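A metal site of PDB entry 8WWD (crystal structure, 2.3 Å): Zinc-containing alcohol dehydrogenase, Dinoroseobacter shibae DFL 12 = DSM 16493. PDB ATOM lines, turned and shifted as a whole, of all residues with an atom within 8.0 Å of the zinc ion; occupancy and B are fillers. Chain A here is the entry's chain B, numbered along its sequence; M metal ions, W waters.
The side-chain amino group (NZ) of Lys 332 lies within salt-bridge range of the side-chain carboxylate (OE1) of Glu 70, at 2.6 Å. The backbone carbonyl oxygen (O) of Glu 70 sits at hydrogen-bond distance from the backbone NH (N) of Gly 45, 2.9 Å away. N of Cys 47 is in hydrogen-bond range of OD2 of Asp 50, at 2.8 Å.
Of the 22 residues printed, 4 come within 4 Å of the zinc ion.
The zinc ion is bound by water W1, OE2 of Glu 70, OE1 of Glu 149, NE2 of His 69 and SG of Cys 47.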
ATOM      1  N   GLY A  45      11.244  -6.860 -12.685  1.00  0.00           N
ATOM      2  CA  GLY A  45      11.231  -6.255 -11.356  1.00  0.00           C
ATOM      3  C   GLY A  45      11.947  -7.146 -10.340  1.00  0.00           C
ATOM      4  O   GLY A  45      12.002  -8.412 -10.524  1.00  0.00           O
ATOM      5  N   ILE A  46      12.469  -6.533  -9.274  1.00  0.00           N
ATOM      6  CA  ILE A  46      13.032  -7.273  -8.104  1.00  0.00           C
ATOM      7  C   ILE A  46      11.921  -7.398  -7.063  1.00  0.00           C
ATOM      8  O   ILE A  46      11.392  -6.374  -6.592  1.00  0.00           O
ATOM      9  CB  ILE A  46      14.276  -6.550  -7.555  1.00  0.00           C
ATOM     10  CG1 ILE A  46      15.390  -6.514  -8.588  1.00  0.00           C
ATOM     11  CG2 ILE A  46      14.753  -7.190  -6.256  1.00  0.00           C
ATOM     12  CD1 ILE A  46      16.449  -5.501  -8.261  1.00  0.00           C
ATOM     13  N   CYS A  47      11.525  -8.623  -6.737  1.00  0.00           N
ATOM     14  CA  CYS A  47      10.408  -8.909  -5.803  1.00  0.00           C
ATOM     15  C   CYS A  47      10.967  -9.275  -4.404  1.00  0.00           C
ATOM     16  O   CYS A  47      12.176  -9.590  -4.284  1.00  0.00           O
ATOM     17  CB  CYS A  47       9.522 -10.016  -6.344  1.00  0.00           C
ATOM     18  SG  CYS A  47       7.916 -10.127  -5.516  1.00  0.00           S
ATOM     19  N   GLY A  48      10.102  -9.253  -3.404  1.00  0.00           N
ATOM     20  CA  GLY A  48      10.402  -9.762  -2.054  1.00  0.00           C
ATOM     21  C   GLY A  48      10.933 -11.182  -2.078  1.00  0.00           C
ATOM     22  O   GLY A  48      11.941 -11.474  -1.379  1.00  0.00           O
ATOM     23  N   SER A  49      10.319 -12.062  -2.870  1.00  0.00           N
ATOM     24  CA  SER A  49      10.743 -13.483  -2.945  1.00  0.00           C
ATOM     25  C   SER A  49      12.203 -13.580  -3.455  1.00  0.00           C
ATOM     26  O   SER A  49      12.933 -14.492  -3.012  1.00  0.00           O
ATOM     27  CB  SER A  49       9.759 -14.299  -3.745  1.00  0.00           C
ATOM     28  OG  SER A  49       9.961 -14.215  -5.151  1.00  0.00           O
ATOM     29  N   ASP A  50      12.649 -12.654  -4.312  1.00  0.00           N
ATOM     30  CA  ASP A  50      14.039 -12.645  -4.853  1.00  0.00           C
ATOM     31  C   ASP A  50      15.034 -12.290  -3.734  1.00  0.00           C
ATOM     32  O   ASP A  50      16.080 -12.945  -3.677  1.00  0.00           O
ATOM     33  CB  ASP A  50      14.178 -11.664  -6.006  1.00  0.00           C
ATOM     34  CG  ASP A  50      13.263 -11.987  -7.173  1.00  0.00           C
ATOM     35  OD1 ASP A  50      13.272 -13.148  -7.607  1.00  0.00           O
ATOM     36  OD2 ASP A  50      12.537 -11.086  -7.597  1.00  0.00           O
ATOM     37  N   GLY A  68      13.920 -13.917 -10.259  1.00  0.00           N
ATOM     38  CA  GLY A  68      13.136 -12.907 -10.988  1.00  0.00           C
ATOM     39  C   GLY A  68      11.897 -13.516 -11.645  1.00  0.00           C
ATOM     40  O   GLY A  68      12.035 -14.582 -12.281  1.00  0.00           O
ATOM     41  N   HIS A  69      10.740 -12.852 -11.494  1.00  0.00           N
ATOM     42  CA  HIS A  69       9.456 -13.364 -12.039  1.00  0.00           C
ATOM     43  C   HIS A  69       8.548 -12.215 -12.499  1.00  0.00           C
ATOM     44  O   HIS A  69       7.356 -12.493 -12.698  1.00  0.00           O
ATOM     45  CB  HIS A  69       8.785 -14.254 -10.974  1.00  0.00           C
ATOM     46  CG  HIS A  69       8.408 -13.511  -9.748  1.00  0.00           C
ATOM     47  ND1 HIS A  69       9.036 -13.685  -8.541  1.00  0.00           N
ATOM     48  CD2 HIS A  69       7.470 -12.557  -9.550  1.00  0.00           C
ATOM     49  CE1 HIS A  69       8.491 -12.882  -7.645  1.00  0.00           C
ATOM     50  NE2 HIS A  69       7.533 -12.164  -8.250  1.00  0.00           N
ATOM     51  N   GLU A  70       9.048 -10.990 -12.608  1.00  0.00           N
ATOM     52  CA  GLU A  70       8.229  -9.789 -12.913  1.00  0.00           C
ATOM     53  C   GLU A  70       8.657  -9.193 -14.261  1.00  0.00           C
ATOM     54  O   GLU A  70       9.087  -8.013 -14.296  1.00  0.00           O
ATOM     55  CB  GLU A  70       8.330  -8.759 -11.787  1.00  0.00           C
ATOM     56  CG  GLU A  70       7.872  -9.283 -10.447  1.00  0.00           C
ATOM     57  CD  GLU A  70       7.961  -8.257  -9.326  1.00  0.00           C
ATOM     58  OE1 GLU A  70       8.602  -7.187  -9.558  1.00  0.00           O
ATOM     59  OE2 GLU A  70       7.388  -8.528  -8.231  1.00  0.00           O
ATOM     60  N   PRO A  89       3.982 -15.149 -14.646  1.00  0.00           N
ATOM     61  CA  PRO A  89       4.961 -16.201 -14.347  1.00  0.00           C
ATOM     62  C   PRO A  89       4.366 -17.497 -13.762  1.00  0.00           C
ATOM     63  O   PRO A  89       5.114 -18.407 -13.584  1.00  0.00           O
ATOM     64  CB  PRO A  89       5.842 -15.506 -13.308  1.00  0.00           C
ATOM     65  CG  PRO A  89       4.883 -14.606 -12.556  1.00  0.00           C
ATOM     66  CD  PRO A  89       4.016 -14.051 -13.667  1.00  0.00           C
ATOM     67  N   ILE A 112       6.093 -21.561 -10.802  1.00  0.00           N
ATOM     68  CA  ILE A 112       6.412 -20.134 -11.088  1.00  0.00           C
ATOM     69  C   ILE A 112       7.816 -20.060 -11.721  1.00  0.00           C
ATOM     70  O   ILE A 112       8.669 -20.918 -11.450  1.00  0.00           O
ATOM     71  CB  ILE A 112       6.272 -19.233  -9.830  1.00  0.00           C
ATOM     72  CG1 ILE A 112       6.160 -17.745 -10.209  1.00  0.00           C
ATOM     73  CG2 ILE A 112       7.393 -19.482  -8.832  1.00  0.00           C
ATOM     74  CD1 ILE A 112       5.824 -16.776  -9.057  1.00  0.00           C
ATOM     75  N   ALA A 146       5.772  -4.240 -16.937  1.00  0.00           N
ATOM     76  CA  ALA A 146       6.479  -5.203 -16.039  1.00  0.00           C
ATOM     77  C   ALA A 146       5.933  -5.145 -14.610  1.00  0.00           C
ATOM     78  O   ALA A 146       6.305  -6.036 -13.831  1.00  0.00           O
ATOM     79  CB  ALA A 146       7.970  -4.931 -16.042  1.00  0.00           C
ATOM     80  N   LEU A 147       5.122  -4.157 -14.240  1.00  0.00           N
ATOM     81  CA  LEU A 147       4.500  -4.086 -12.892  1.00  0.00           C
ATOM     82  C   LEU A 147       3.288  -5.013 -12.794  1.00  0.00           C
ATOM     83  O   LEU A 147       2.681  -5.037 -11.700  1.00  0.00           O
ATOM     84  CB  LEU A 147       4.095  -2.654 -12.574  1.00  0.00           C
ATOM     85  CG  LEU A 147       5.271  -1.692 -12.434  1.00  0.00           C
ATOM     86  CD1 LEU A 147       4.781  -0.263 -12.221  1.00  0.00           C
ATOM     87  CD2 LEU A 147       6.168  -2.142 -11.288  1.00  0.00           C
ATOM     88  N   ALA A 148       2.913  -5.731 -13.857  1.00  0.00           N
ATOM     89  CA  ALA A 148       1.597  -6.423 -13.916  1.00  0.00           C
ATOM     90  C   ALA A 148       1.534  -7.434 -12.789  1.00  0.00           C
ATOM     91  O   ALA A 148       0.524  -7.469 -12.058  1.00  0.00           O
ATOM     92  CB  ALA A 148       1.361  -7.038 -15.275  1.00  0.00           C
ATOM     93  N   GLU A 149       2.588  -8.228 -12.616  1.00  0.00           N
ATOM     94  CA  GLU A 149       2.588  -9.305 -11.591  1.00  0.00           C
ATOM     95  C   GLU A 149       2.486  -8.722 -10.180  1.00  0.00           C
ATOM     96  O   GLU A 149       1.567  -9.093  -9.451  1.00  0.00           O
ATOM     97  CB  GLU A 149       3.798 -10.210 -11.753  1.00  0.00           C
ATOM     98  CG  GLU A 149       3.687 -11.445 -10.874  1.00  0.00           C
ATOM     99  CD  GLU A 149       4.306 -11.381  -9.487  1.00  0.00           C
ATOM    100  OE1 GLU A 149       4.952 -10.365  -9.069  1.00  0.00           O
ATOM    101  OE2 GLU A 149       4.178 -12.416  -8.813  1.00  0.00           O
ATOM    102  N   PRO A 150       3.375  -7.835  -9.720  1.00  0.00           N
ATOM    103  CA  PRO A 150       3.240  -7.264  -8.377  1.00  0.00           C
ATOM    104  C   PRO A 150       1.884  -6.576  -8.165  1.00  0.00           C
ATOM    105  O   PRO A 150       1.317  -6.702  -7.107  1.00  0.00           O
ATOM    106  CB  PRO A 150       4.372  -6.251  -8.228  1.00  0.00           C
ATOM    107  CG  PRO A 150       4.938  -6.082  -9.641  1.00  0.00           C
ATOM    108  CD  PRO A 150       4.583  -7.349 -10.392  1.00  0.00           C
ATOM    109  N   VAL A 151       1.361  -5.926  -9.202  1.00  0.00           N
ATOM    110  CA  VAL A 151       0.058  -5.233  -9.026  1.00  0.00           C
ATOM    111  C   VAL A 151      -1.012  -6.328  -8.940  1.00  0.00           C
ATOM    112  O   VAL A 151      -1.903  -6.194  -8.090  1.00  0.00           O
ATOM    113  CB  VAL A 151      -0.258  -4.182 -10.100  1.00  0.00           C
ATOM    114  CG1 VAL A 151      -1.632  -3.569  -9.860  1.00  0.00           C
ATOM    115  CG2 VAL A 151       0.816  -3.098 -10.167  1.00  0.00           C
ATOM    116  N   VAL A 153      -1.065  -9.194  -7.689  1.00  0.00           N
ATOM    117  CA  VAL A 153      -1.077  -9.757  -6.310  1.00  0.00           C
ATOM    118  C   VAL A 153      -2.076  -8.974  -5.438  1.00  0.00           C
ATOM    119  O   VAL A 153      -2.981  -9.603  -4.785  1.00  0.00           O
ATOM    120  CB  VAL A 153       0.315  -9.738  -5.675  1.00  0.00           C
ATOM    121  CG1 VAL A 153       0.260 -10.079  -4.198  1.00  0.00           C
ATOM    122  CG2 VAL A 153       1.273 -10.682  -6.389  1.00  0.00           C
ATOM    123  N   ALA A 180       5.927  -2.075  -2.544  1.00  0.00           N
ATOM    124  CA  ALA A 180       5.210  -2.396  -3.787  1.00  0.00           C
ATOM    125  C   ALA A 180       3.860  -2.991  -3.426  1.00  0.00           C
ATOM    126  O   ALA A 180       2.877  -2.561  -4.026  1.00  0.00           O
ATOM    127  CB  ALA A 180       6.016  -3.322  -4.653  1.00  0.00           C
ATOM    128  N   ILE A 181       3.768  -3.909  -2.465  1.00  0.00           N
ATOM    129  CA  ILE A 181       2.471  -4.572  -2.137  1.00  0.00           C
ATOM    130  C   ILE A 181       1.424  -3.525  -1.708  1.00  0.00           C
ATOM    131  O   ILE A 181       0.251  -3.586  -2.195  1.00  0.00           O
ATOM    132  CB  ILE A 181       2.619  -5.680  -1.075  1.00  0.00           C
ATOM    133  CG1 ILE A 181       3.384  -6.892  -1.620  1.00  0.00           C
ATOM    134  CG2 ILE A 181       1.243  -6.064  -0.531  1.00  0.00           C
ATOM    135  CD1 ILE A 181       3.997  -7.778  -0.530  1.00  0.00           C
ATOM    136  N   TYR A 285      -2.585 -14.561  -7.216  1.00  0.00           N
ATOM    137  CA  TYR A 285      -3.653 -14.009  -8.084  1.00  0.00           C
ATOM    138  C   TYR A 285      -4.058 -15.086  -9.072  1.00  0.00           C
ATOM    139  O   TYR A 285      -3.250 -16.011  -9.307  1.00  0.00           O
ATOM    140  CB  TYR A 285      -3.139 -12.792  -8.838  1.00  0.00           C
ATOM    141  CG  TYR A 285      -1.842 -13.069  -9.565  1.00  0.00           C
ATOM    142  CD1 TYR A 285      -0.623 -12.933  -8.935  1.00  0.00           C
ATOM    143  CD2 TYR A 285      -1.861 -13.551 -10.860  1.00  0.00           C
ATOM    144  CE1 TYR A 285       0.568 -13.220  -9.590  1.00  0.00           C
ATOM    145  CE2 TYR A 285      -0.688 -13.840 -11.528  1.00  0.00           C
ATOM    146  CZ  TYR A 285       0.522 -13.689 -10.887  1.00  0.00           C
ATOM    147  OH  TYR A 285       1.651 -13.958 -11.581  1.00  0.00           O
ATOM    148  N   LYS A 332      10.137  -0.071  -6.137  1.00  0.00           N
ATOM    149  CA  LYS A 332      10.335  -1.156  -7.124  1.00  0.00           C
ATOM    150  C   LYS A 332      11.545  -0.811  -7.980  1.00  0.00           C
ATOM    151  O   LYS A 332      11.583   0.296  -8.529  1.00  0.00           O
ATOM    152  CB  LYS A 332       9.093  -1.331  -8.001  1.00  0.00           C
ATOM    153  CG  LYS A 332       9.186  -2.438  -9.048  1.00  0.00           C
ATOM    154  CD  LYS A 332       9.465  -3.821  -8.478  1.00  0.00           C
ATOM    155  CE  LYS A 332       8.352  -4.361  -7.599  1.00  0.00           C
ATOM    156  NZ  LYS A 332       8.465  -5.823  -7.365  1.00  0.00           N
HETATM  157 ZN    ZN M   1       6.449 -10.254  -7.520  1.00  0.00          ZN
HETATM  158  O   HOH W   1       4.783 -10.382  -6.351  1.00  0.00           O
